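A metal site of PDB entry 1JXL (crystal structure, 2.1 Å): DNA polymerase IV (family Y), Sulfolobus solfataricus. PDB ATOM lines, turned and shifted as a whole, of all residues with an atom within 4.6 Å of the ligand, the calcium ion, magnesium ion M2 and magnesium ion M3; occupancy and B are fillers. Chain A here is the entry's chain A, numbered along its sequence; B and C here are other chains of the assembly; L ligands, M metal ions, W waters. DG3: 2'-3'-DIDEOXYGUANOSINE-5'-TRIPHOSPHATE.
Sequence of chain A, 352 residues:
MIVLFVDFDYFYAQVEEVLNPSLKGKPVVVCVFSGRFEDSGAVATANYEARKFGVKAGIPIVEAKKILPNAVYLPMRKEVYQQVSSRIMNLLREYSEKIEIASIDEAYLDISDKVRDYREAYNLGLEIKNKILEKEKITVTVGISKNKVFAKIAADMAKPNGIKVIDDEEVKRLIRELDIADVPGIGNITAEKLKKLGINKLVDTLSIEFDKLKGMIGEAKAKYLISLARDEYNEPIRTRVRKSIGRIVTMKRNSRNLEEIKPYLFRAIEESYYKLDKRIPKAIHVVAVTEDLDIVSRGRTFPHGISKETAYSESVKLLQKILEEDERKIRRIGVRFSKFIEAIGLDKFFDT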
ATOM      1  N   ASP A   7      13.920  -8.965  22.048  1.00  0.00           N
ATOM      2  CA  ASP A   7      12.631  -9.050  21.393  1.00  0.00           C
ATOM      3  C   ASP A   7      12.251  -7.646  20.909  1.00  0.00           C
ATOM      4  O   ASP A   7      11.980  -6.744  21.719  1.00  0.00           O
ATOM      5  CB  ASP A   7      11.594  -9.529  22.401  1.00  0.00           C
ATOM      6  CG  ASP A   7      10.242  -9.790  21.777  1.00  0.00           C
ATOM      7  OD1 ASP A   7       9.697  -8.927  21.031  1.00  0.00           O
ATOM      8  OD2 ASP A   7       9.690 -10.877  22.078  1.00  0.00           O
ATOM      9  N   PHE A   8      12.192  -7.444  19.582  1.00  0.00           N
ATOM     10  CA  PHE A   8      11.885  -6.085  19.118  1.00  0.00           C
ATOM     11  C   PHE A   8      10.433  -5.658  19.427  1.00  0.00           C
ATOM     12  O   PHE A   8       9.523  -6.384  19.128  1.00  0.00           O
ATOM     13  CB  PHE A   8      12.133  -5.984  17.607  1.00  0.00           C
ATOM     14  CG  PHE A   8      13.393  -6.672  17.121  1.00  0.00           C
ATOM     15  CD1 PHE A   8      14.503  -6.821  17.941  1.00  0.00           C
ATOM     16  CD2 PHE A   8      13.498  -7.069  15.792  1.00  0.00           C
ATOM     17  CE1 PHE A   8      15.680  -7.332  17.465  1.00  0.00           C
ATOM     18  CE2 PHE A   8      14.709  -7.575  15.306  1.00  0.00           C
ATOM     19  CZ  PHE A   8      15.790  -7.703  16.163  1.00  0.00           C
ATOM     20  N   ASP A   9      10.211  -4.479  19.979  1.00  0.00           N
ATOM     21  CA  ASP A   9       8.841  -4.059  20.296  1.00  0.00           C
ATOM     22  C   ASP A   9       7.870  -3.840  19.117  1.00  0.00           C
ATOM     23  O   ASP A   9       8.217  -3.172  18.150  1.00  0.00           O
ATOM     24  CB  ASP A   9       8.861  -2.773  21.141  1.00  0.00           C
ATOM     25  CG  ASP A   9       9.760  -2.897  22.411  1.00  0.00           C
ATOM     26  OD1 ASP A   9       9.705  -3.935  23.099  1.00  0.00           O
ATOM     27  OD2 ASP A   9      10.495  -1.942  22.741  1.00  0.00           O
ATOM     28  N   TYR A  10       6.651  -4.380  19.218  1.00  0.00           N
ATOM     29  CA  TYR A  10       5.618  -4.237  18.184  1.00  0.00           C
ATOM     30  C   TYR A  10       6.296  -4.051  16.789  1.00  0.00           C
ATOM     31  O   TYR A  10       5.936  -3.136  16.016  1.00  0.00           O
ATOM     32  CB  TYR A  10       4.644  -3.066  18.597  1.00  0.00           C
ATOM     33  CG  TYR A  10       5.200  -1.637  18.735  1.00  0.00           C
ATOM     34  CD1 TYR A  10       5.014  -0.684  17.706  1.00  0.00           C
ATOM     35  CD2 TYR A  10       5.919  -1.224  19.882  1.00  0.00           C
ATOM     36  CE1 TYR A  10       5.534   0.654  17.807  1.00  0.00           C
ATOM     37  CE2 TYR A  10       6.443   0.119  19.995  1.00  0.00           C
ATOM     38  CZ  TYR A  10       6.240   1.036  18.955  1.00  0.00           C
ATOM     39  OH  TYR A  10       6.713   2.353  19.068  1.00  0.00           O
ATOM     40  N   PHE A  11       7.307  -4.907  16.509  1.00  0.00           N
ATOM     41  CA  PHE A  11       8.085  -4.799  15.293  1.00  0.00           C
ATOM     42  C   PHE A  11       7.540  -4.250  14.008  1.00  0.00           C
ATOM     43  O   PHE A  11       8.043  -3.212  13.559  1.00  0.00           O
ATOM     44  CB  PHE A  11       8.838  -6.124  15.003  1.00  0.00           C
ATOM     45  CG  PHE A  11      10.065  -5.918  14.138  1.00  0.00           C
ATOM     46  CD1 PHE A  11      10.908  -4.855  14.394  1.00  0.00           C
ATOM     47  CD2 PHE A  11      10.300  -6.707  12.999  1.00  0.00           C
ATOM     48  CE1 PHE A  11      11.988  -4.579  13.539  1.00  0.00           C
ATOM     49  CE2 PHE A  11      11.391  -6.443  12.131  1.00  0.00           C
ATOM     50  CZ  PHE A  11      12.224  -5.369  12.400  1.00  0.00           C
ATOM     51  N   TYR A  12       6.517  -4.885  13.432  1.00  0.00           N
ATOM     52  CA  TYR A  12       5.946  -4.427  12.162  1.00  0.00           C
ATOM     53  C   TYR A  12       5.375  -2.996  12.235  1.00  0.00           C
ATOM     54  O   TYR A  12       5.719  -2.186  11.387  1.00  0.00           O
ATOM     55  CB  TYR A  12       4.874  -5.378  11.598  1.00  0.00           C
ATOM     56  CG  TYR A  12       5.290  -6.834  11.381  1.00  0.00           C
ATOM     57  CD1 TYR A  12       6.614  -7.229  11.533  1.00  0.00           C
ATOM     58  CD2 TYR A  12       4.338  -7.824  11.039  1.00  0.00           C
ATOM     59  CE1 TYR A  12       7.012  -8.556  11.357  1.00  0.00           C
ATOM     60  CE2 TYR A  12       4.718  -9.175  10.870  1.00  0.00           C
ATOM     61  CZ  TYR A  12       6.077  -9.526  11.041  1.00  0.00           C
ATOM     62  OH  TYR A  12       6.495 -10.846  10.937  1.00  0.00           O
ATOM     63  N   VAL A  32      -3.185  -8.061   7.457  1.00  0.00           N
ATOM     64  CA  VAL A  32      -3.018  -9.042   6.405  1.00  0.00           C
ATOM     65  C   VAL A  32      -4.386  -9.115   5.754  1.00  0.00           C
ATOM     66  O   VAL A  32      -5.303  -9.784   6.297  1.00  0.00           O
ATOM     67  CB  VAL A  32      -2.697 -10.426   6.964  1.00  0.00           C
ATOM     68  CG1 VAL A  32      -2.571 -11.439   5.801  1.00  0.00           C
ATOM     69  CG2 VAL A  32      -1.422 -10.365   7.785  1.00  0.00           C
ATOM     70  N   VAL A  43      -5.502  -8.882  11.765  1.00  0.00           N
ATOM     71  CA  VAL A  43      -4.530  -7.925  12.261  1.00  0.00           C
ATOM     72  C   VAL A  43      -3.268  -8.738  12.539  1.00  0.00           C
ATOM     73  O   VAL A  43      -3.328  -9.691  13.332  1.00  0.00           O
ATOM     74  CB  VAL A  43      -4.959  -7.316  13.584  1.00  0.00           C
ATOM     75  CG1 VAL A  43      -3.727  -6.669  14.234  1.00  0.00           C
ATOM     76  CG2 VAL A  43      -6.152  -6.304  13.366  1.00  0.00           C
ATOM     77  N   ALA A  44      -2.160  -8.377  11.879  1.00  0.00           N
ATOM     78  CA  ALA A  44      -0.848  -9.057  12.060  1.00  0.00           C
ATOM     79  C   ALA A  44      -0.242  -8.528  13.370  1.00  0.00           C
ATOM     80  O   ALA A  44       0.251  -9.324  14.217  1.00  0.00           O
ATOM     81  CB  ALA A  44       0.124  -8.743  10.840  1.00  0.00           C
ATOM     82  N   THR A  45      -0.212  -7.196  13.516  1.00  0.00           N
ATOM     83  CA  THR A  45       0.224  -6.612  14.769  1.00  0.00           C
ATOM     84  C   THR A  45      -0.209  -5.139  14.958  1.00  0.00           C
ATOM     85  O   THR A  45      -0.573  -4.484  14.027  1.00  0.00           O
ATOM     86  CB  THR A  45       1.737  -6.688  14.938  1.00  0.00           C
ATOM     87  OG1 THR A  45       2.063  -6.195  16.250  1.00  0.00           O
ATOM     88  CG2 THR A  45       2.427  -5.811  13.954  1.00  0.00           C
ATOM     89  N   TYR A  48       1.256  -0.085  20.729  1.00  0.00           N
ATOM     90  CA  TYR A  48       0.636   0.067  22.051  1.00  0.00           C
ATOM     91  C   TYR A  48      -0.614   0.922  22.100  1.00  0.00           C
ATOM     92  O   TYR A  48      -1.555   0.568  22.791  1.00  0.00           O
ATOM     93  CB  TYR A  48       1.661   0.542  23.066  1.00  0.00           C
ATOM     94  CG  TYR A  48       2.575  -0.612  23.382  1.00  0.00           C
ATOM     95  CD1 TYR A  48       3.736  -0.835  22.619  1.00  0.00           C
ATOM     96  CD2 TYR A  48       2.190  -1.586  24.300  1.00  0.00           C
ATOM     97  CE1 TYR A  48       4.455  -2.001  22.763  1.00  0.00           C
ATOM     98  CE2 TYR A  48       2.908  -2.740  24.463  1.00  0.00           C
ATOM     99  CZ  TYR A  48       4.025  -2.938  23.690  1.00  0.00           C
ATOM    100  OH  TYR A  48       4.696  -4.143  23.880  1.00  0.00           O
ATOM    101  N   ARG A  51      -3.181  -1.416  20.914  1.00  0.00           N
ATOM    102  CA  ARG A  51      -3.403  -2.529  21.864  1.00  0.00           C
ATOM    103  C   ARG A  51      -4.081  -2.074  23.133  1.00  0.00           C
ATOM    104  O   ARG A  51      -4.866  -2.796  23.686  1.00  0.00           O
ATOM    105  CB  ARG A  51      -2.078  -3.258  22.209  1.00  0.00           C
ATOM    106  CG  ARG A  51      -1.507  -4.008  21.029  1.00  0.00           C
ATOM    107  CD  ARG A  51      -0.909  -5.363  21.312  1.00  0.00           C
ATOM    108  NE  ARG A  51       0.144  -5.536  20.312  1.00  0.00           N
ATOM    109  CZ  ARG A  51       1.292  -6.199  20.461  1.00  0.00           C
ATOM    110  NH1 ARG A  51       1.582  -6.791  21.603  1.00  0.00           N
ATOM    111  NH2 ARG A  51       2.142  -6.302  19.428  1.00  0.00           N
ATOM    112  N   ALA A  57      -2.963  -8.581  17.484  1.00  0.00           N
ATOM    113  CA  ALA A  57      -2.712  -9.656  16.504  1.00  0.00           C
ATOM    114  C   ALA A  57      -3.804 -10.725  16.635  1.00  0.00           C
ATOM    115  O   ALA A  57      -4.196 -11.090  17.759  1.00  0.00           O
ATOM    116  CB  ALA A  57      -1.328 -10.319  16.772  1.00  0.00           C
ATOM    117  N   GLY A  58      -4.315 -11.175  15.497  1.00  0.00           N
ATOM    118  CA  GLY A  58      -5.307 -12.240  15.515  1.00  0.00           C
ATOM    119  C   GLY A  58      -6.763 -11.877  15.290  1.00  0.00           C
ATOM    120  O   GLY A  58      -7.504 -12.698  14.757  1.00  0.00           O
ATOM    121  N   ASP A 105      11.770 -11.192  14.855  1.00  0.00           N
ATOM    122  CA  ASP A 105      12.027 -10.162  15.866  1.00  0.00           C
ATOM    123  C   ASP A 105      12.555 -10.649  17.206  1.00  0.00           C
ATOM    124  O   ASP A 105      12.351  -9.971  18.191  1.00  0.00           O
ATOM    125  CB  ASP A 105      10.755  -9.349  16.106  1.00  0.00           C
ATOM    126  CG  ASP A 105       9.792 -10.103  16.922  1.00  0.00           C
ATOM    127  OD1 ASP A 105       9.774 -11.298  16.679  1.00  0.00           O
ATOM    128  OD2 ASP A 105       9.117  -9.549  17.779  1.00  0.00           O
ATOM    129  N   GLU A 106      13.207 -11.821  17.242  1.00  0.00           N
ATOM    130  CA  GLU A 106      13.714 -12.384  18.495  1.00  0.00           C
ATOM    131  C   GLU A 106      15.059 -13.091  18.324  1.00  0.00           C
ATOM    132  O   GLU A 106      15.255 -13.857  17.350  1.00  0.00           O
ATOM    133  CB  GLU A 106      12.718 -13.418  19.025  1.00  0.00           C
ATOM    134  CG  GLU A 106      11.398 -12.823  19.409  1.00  0.00           C
ATOM    135  CD  GLU A 106      10.467 -13.854  20.017  1.00  0.00           C
ATOM    136  OE1 GLU A 106      10.920 -14.985  20.343  1.00  0.00           O
ATOM    137  OE2 GLU A 106       9.285 -13.526  20.205  1.00  0.00           O
ATOM    138  N   LYS A 152      13.318 -15.321  28.168  1.00  0.00           N
ATOM    139  CA  LYS A 152      12.164 -14.894  27.374  1.00  0.00           C
ATOM    140  C   LYS A 152      11.064 -14.444  28.305  1.00  0.00           C
ATOM    141  O   LYS A 152      10.402 -13.437  28.053  1.00  0.00           O
ATOM    142  CB  LYS A 152      11.649 -16.054  26.498  1.00  0.00           C
ATOM    143  CG  LYS A 152      10.327 -15.775  25.723  1.00  0.00           C
ATOM    144  CD  LYS A 152      10.222 -16.729  24.484  1.00  0.00           C
ATOM    145  CE  LYS A 152       9.071 -16.405  23.506  1.00  0.00           C
ATOM    146  NZ  LYS A 152       9.192 -15.051  22.865  1.00  0.00           N
ATOM    147  N   LYS A 159       8.258  -6.083  28.695  1.00  0.00           N
ATOM    148  CA  LYS A 159       7.926  -5.322  27.494  1.00  0.00           C
ATOM    149  C   LYS A 159       6.826  -4.337  27.759  1.00  0.00           C
ATOM    150  O   LYS A 159       5.945  -4.597  28.536  1.00  0.00           O
ATOM    151  CB  LYS A 159       7.612  -6.260  26.295  1.00  0.00           C
ATOM    152  CG  LYS A 159       6.401  -7.180  26.402  1.00  0.00           C
ATOM    153  CD  LYS A 159       6.173  -7.954  25.060  1.00  0.00           C
ATOM    154  CE  LYS A 159       7.345  -8.893  24.670  1.00  0.00           C
ATOM    155  NZ  LYS A 159       7.044  -9.751  23.471  1.00  0.00           N
ATOM    156  P    DC B   3      -9.454 -14.479   6.018  1.00  0.00           P
ATOM    157  OP1  DC B   3     -10.128 -13.946   4.801  1.00  0.00           O
ATOM    158  OP2  DC B   3      -9.453 -15.938   6.304  1.00  0.00           O
ATOM    159  O5'  DC B   3      -7.952 -13.984   5.927  1.00  0.00           O
ATOM    160  C5'  DC B   3      -7.136 -13.942   7.078  1.00  0.00           C
ATOM    161  C4'  DC B   3      -5.727 -13.633   6.649  1.00  0.00           C
ATOM    162  O4'  DC B   3      -4.920 -13.214   7.764  1.00  0.00           O
ATOM    163  C3'  DC B   3      -4.997 -14.799   6.012  1.00  0.00           C
ATOM    164  O3'  DC B   3      -4.157 -14.238   4.995  1.00  0.00           O
ATOM    165  C2'  DC B   3      -4.211 -15.394   7.183  1.00  0.00           C
ATOM    166  C1'  DC B   3      -3.921 -14.163   8.054  1.00  0.00           C
ATOM    167  N1   DC B   3      -3.984 -14.402   9.506  1.00  0.00           N
ATOM    168  C2   DC B   3      -2.885 -14.077  10.310  1.00  0.00           C
ATOM    169  O2   DC B   3      -1.878 -13.551   9.779  1.00  0.00           O
ATOM    170  N3   DC B   3      -2.966 -14.332  11.654  1.00  0.00           N
ATOM    171  C4   DC B   3      -4.079 -14.867  12.173  1.00  0.00           C
ATOM    172  N4   DC B   3      -4.109 -15.110  13.468  1.00  0.00           N
ATOM    173  C5   DC B   3      -5.203 -15.181  11.370  1.00  0.00           C
ATOM    174  C6   DC B   3      -5.124 -14.931  10.060  1.00  0.00           C
ATOM    175  P    DG B   4      -3.421 -15.197   3.944  1.00  0.00           P
ATOM    176  OP1  DG B   4      -3.047 -14.387   2.747  1.00  0.00           O
ATOM    177  OP2  DG B   4      -4.252 -16.427   3.771  1.00  0.00           O
ATOM    178  O5'  DG B   4      -2.094 -15.568   4.712  1.00  0.00           O
ATOM    179  C5'  DG B   4      -1.155 -14.553   5.023  1.00  0.00           C
ATOM    180  C4'  DG B   4      -0.036 -15.144   5.829  1.00  0.00           C
ATOM    181  O4'  DG B   4      -0.413 -15.336   7.229  1.00  0.00           O
ATOM    182  C3'  DG B   4       0.369 -16.523   5.302  1.00  0.00           C
ATOM    183  O3'  DG B   4       1.760 -16.588   5.350  1.00  0.00           O
ATOM    184  C2'  DG B   4      -0.195 -17.486   6.319  1.00  0.00           C
ATOM    185  C1'  DG B   4      -0.121 -16.671   7.613  1.00  0.00           C
ATOM    186  N9   DG B   4      -1.078 -17.079   8.635  1.00  0.00           N
ATOM    187  C8   DG B   4      -2.306 -17.656   8.421  1.00  0.00           C
ATOM    188  N7   DG B   4      -2.922 -17.983   9.525  1.00  0.00           N
ATOM    189  C5   DG B   4      -2.066 -17.587  10.528  1.00  0.00           C
ATOM    190  C6   DG B   4      -2.208 -17.673  11.951  1.00  0.00           C
ATOM    191  O6   DG B   4      -3.164 -18.125  12.611  1.00  0.00           O
ATOM    192  N1   DG B   4      -1.102 -17.168  12.600  1.00  0.00           N
ATOM    193  C2   DG B   4      -0.009 -16.634  11.974  1.00  0.00           C
ATOM    194  N2   DG B   4       0.936 -16.203  12.782  1.00  0.00           N
ATOM    195  N3   DG B   4       0.138 -16.527  10.659  1.00  0.00           N
ATOM    196  C4   DG B   4      -0.923 -17.019  10.002  1.00  0.00           C
ATOM    197  P    DT C  12       3.173 -20.456  22.708  1.00  0.00           P
ATOM    198  OP1  DT C  12       3.962 -20.358  23.959  1.00  0.00           O
ATOM    199  OP2  DT C  12       1.748 -20.038  22.736  1.00  0.00           O
ATOM    200  O5'  DT C  12       3.921 -19.612  21.600  1.00  0.00           O
ATOM    201  C5'  DT C  12       5.256 -19.948  21.166  1.00  0.00           C
ATOM    202  C4'  DT C  12       5.672 -19.015  20.045  1.00  0.00           C
ATOM    203  O4'  DT C  12       5.082 -19.441  18.780  1.00  0.00           O
ATOM    204  C3'  DT C  12       5.248 -17.557  20.239  1.00  0.00           C
ATOM    205  O3'  DT C  12       6.323 -16.670  19.901  1.00  0.00           O
ATOM    206  C2'  DT C  12       4.110 -17.375  19.259  1.00  0.00           C
ATOM    207  C1'  DT C  12       4.500 -18.323  18.132  1.00  0.00           C
ATOM    208  N1   DT C  12       3.403 -18.847  17.260  1.00  0.00           N
ATOM    209  C2   DT C  12       3.716 -19.179  15.924  1.00  0.00           C
ATOM    210  O2   DT C  12       4.830 -19.106  15.434  1.00  0.00           O
ATOM    211  N3   DT C  12       2.654 -19.618  15.187  1.00  0.00           N
ATOM    212  C4   DT C  12       1.366 -19.813  15.608  1.00  0.00           C
ATOM    213  O4   DT C  12       0.538 -20.227  14.813  1.00  0.00           O
ATOM    214  C5   DT C  12       1.107 -19.486  17.020  1.00  0.00           C
ATOM    215  C7   DT C  12      -0.269 -19.696  17.587  1.00  0.00           C
ATOM    216  C6   DT C  12       2.128 -18.999  17.745  1.00  0.00           C
HETATM  217  PG  DG3 L   1       5.067  -7.894  18.342  1.00  0.00           P
HETATM  218  O1G DG3 L   1       4.378  -7.636  19.624  1.00  0.00           O
HETATM  219  O2G DG3 L   1       6.512  -7.483  18.144  1.00  0.00           O
HETATM  220  O3G DG3 L   1       4.186  -7.485  17.048  1.00  0.00           O
HETATM  221  O3B DG3 L   1       4.940  -9.477  18.548  1.00  0.00           O
HETATM  222  PB  DG3 L   1       5.354 -10.202  19.921  1.00  0.00           P
HETATM  223  O1B DG3 L   1       4.489  -9.523  20.876  1.00  0.00           O
HETATM  224  O2B DG3 L   1       6.806 -10.357  19.989  1.00  0.00           O
HETATM  225  O3A DG3 L   1       4.615 -11.598  19.611  1.00  0.00           O
HETATM  226  PA  DG3 L   1       5.017 -13.044  18.940  1.00  0.00           P
HETATM  227  O1A DG3 L   1       3.706 -13.744  19.208  1.00  0.00           O
HETATM  228  O2A DG3 L   1       6.311 -13.545  19.537  1.00  0.00           O
HETATM  229  O5' DG3 L   1       5.235 -12.849  17.354  1.00  0.00           O
HETATM  230  C5' DG3 L   1       6.429 -12.515  16.582  1.00  0.00           C
HETATM  231  C4' DG3 L   1       6.033 -11.940  15.218  1.00  0.00           C
HETATM  232  O4' DG3 L   1       4.791 -12.530  14.663  1.00  0.00           O
HETATM  233  C3' DG3 L   1       5.787 -10.421  15.199  1.00  0.00           C
HETATM  234  C2' DG3 L   1       4.260 -10.300  15.275  1.00  0.00           C
HETATM  235  C1' DG3 L   1       3.785 -11.531  14.479  1.00  0.00           C
HETATM  236  N9  DG3 L   1       2.517 -12.146  14.888  1.00  0.00           N
HETATM  237  C8  DG3 L   1       2.013 -12.442  16.158  1.00  0.00           C
HETATM  238  N7  DG3 L   1       0.803 -12.972  16.150  1.00  0.00           N
HETATM  239  C5  DG3 L   1       0.466 -12.937  14.789  1.00  0.00           C
HETATM  240  C6  DG3 L   1      -0.771 -13.233  14.083  1.00  0.00           C
HETATM  241  O6  DG3 L   1      -1.810 -13.622  14.637  1.00  0.00           O
HETATM  242  N1  DG3 L   1      -0.704 -13.054  12.658  1.00  0.00           N
HETATM  243  C2  DG3 L   1       0.459 -12.656  11.975  1.00  0.00           C
HETATM  244  N2  DG3 L   1       0.450 -12.533  10.633  1.00  0.00           N
HETATM  245  N3  DG3 L   1       1.604 -12.391  12.621  1.00  0.00           N
HETATM  246  C4  DG3 L   1       1.544 -12.532  13.987  1.00  0.00           C
HETATM  247 CA    CA M   1       8.184  -8.357  19.444  1.00  0.00          CA
HETATM  248 MG    MG M   2       8.512 -11.766  19.920  1.00  0.00          MG
HETATM  249 MG    MG M   3       5.169  -7.216  21.299  1.00  0.00          MG
HETATM  250  O   HOH W   1       7.108  -7.759  21.471  1.00  0.00           O
HETATM  251  O   HOH W   2       2.384 -10.179  22.333  1.00  0.00           O
HETATM  252  O   HOH W   3       1.823  -8.976  17.381  1.00  0.00           O
HETATM  253  O   HOH W   4       4.057 -12.305  11.138  1.00  0.00           O
HETATM  254  O   HOH W   5       5.440  -7.389  14.582  1.00  0.00           O
HETATM  255  O   HOH W   6       3.709  -8.379  23.275  1.00  0.00           O
HETATM  256  O   HOH W   7       2.016 -10.538  19.737  1.00  0.00           O
HETATM  257  O   HOH W   8       8.191 -14.487  17.744  1.00  0.00           O
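The side-chain carboxylate (OE1) of Glu 106 is in salt-bridge range of the side-chain amino group (NZ) of Lys 152 (3.1 Å).
OD2 of Asp 7 lies within salt-bridge range of NZ of Lys 159 (3.2 Å).
The side-chain hydroxyl (OG1) of Thr 45 lies within hydrogen-bond range of the guanidinium group (NH2) of Arg 51 (3.2 Å).
The backbone NH (N) of Gly 58 is in hydrogen-bond range of the backbone carbonyl oxygen (O) of Val 43, 2.8 Å away.
The calcium ion is bound by the side-chain carboxylate (OD2) of Asp 105 (2.3 Å), the side-chain carboxylate (OD1) of Asp 7 (2.3 Å), an oxygen (O2G) of the ligand (2.3 Å), water W1 (2.4 Å), the backbone carbonyl oxygen (O) of Phe 8 (2.4 Å) and an oxygen (O2B) of the ligand (2.5 Å).
Water W5 lies within hydrogen-bond range of O3G of the ligand (2.8 Å) and N of Tyr 12 of chain A (3.0 Å).
Water W3 lies within hydrogen-bond range of O3G of the ligand (2.8 Å), OG1 of Thr 45 (3.0 Å) and NH2 of Arg 51 (3.4 Å).
Water W4 bridges the side-chain hydroxyl (OH) of Tyr 12 of chain A and a nitrogen (N3) of the ligand.
Residues that only touch magnesium ion M3: Arg 51 (3.6 Å), Tyr 10 (3.8 Å) and Lys 159 (3.8 Å).
Along chain A the residues within 4 Å of magnesium ion M3 span positions 10 to 159.
Three residues have an atom within 4 Å of the calcium ion: Asp 7, Phe 8 and Asp 105.
The nearest printed residue that does not touch the calcium ion is Tyr 10 (4.3 Å).
OG1 of Thr 45 is in hydrogen-bond range of O3G of the ligand, 2.6 Å away.
NH2 of Arg 51 is in salt-bridge range of O3G of the ligand, 3.4 Å away.
A nitrogen (N2) of the ligand is in hydrogen-bond range of O2 of DC 3 of chain B, at 2.7 Å.
The backbone NH (N) of Phe 11 sits close to an oxygen (O2G) of the ligand, 3.2 Å away.
The backbone NH of Tyr 10 sits close to an oxygen (O2G) of the ligand (3.3 Å).
The side-chain amino group (NZ) of Lys 159 sits close to an oxygen (O2B) of the ligand (3.5 Å).
An oxygen (O2A) of the ligand sits close to O3' of DT 12 of chain C.
Ala 44 touches the ligand (O to C4, 3.5 Å).
Ala 57 touches the ligand (CB to N7, 3.5 Å).
Gly 58 touches the ligand (N to O6, 3.6 Å).
N2 of DG 4 of chain B touches N1 of the ligand, at 3.6 Å.
Hydrophobic or aromatic side chains that line the ligand: Ala 44 and Ala 57.
15 residues have an atom within 4 Å of the ligand: Asp 7, Phe 8, Tyr 10, Phe 11, Ala 44, Thr 45, Arg 51, Ala 57, Gly 58, Asp 105, Glu 106, Lys 159, DC 3 of chain B, DG 4 of chain B and DT 12 of chain C.
The nearest printed residue that does not touch the ligand is Asp 9 (4.01 Å).
Magnesium ion M3 is bound by O1G of the ligand (1.9 Å), water W1 (2.0 Å) and O1B of the ligand (2.4 Å).
Magnesium ion M3 has three donor atoms within binding distance.
Slightly farther from magnesium ion M3 lies water W6 (2.7 Å).
Magnesium ion M2 is bound by the side-chain carboxylate (OE2) of Glu 106, 1.9 Å away.
O2B of the ligand binds magnesium ion M2 (2.2 Å).
Magnesium ion M2 has two donor atoms within binding distance.
Slightly farther from magnesium ion M2 lies the side-chain carboxylate (OD2) of Asp 7 (2.6 Å).
Three residues have an atom within 4 Å of magnesium ion M2: Asp 7, Asp 105 and Glu 106.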
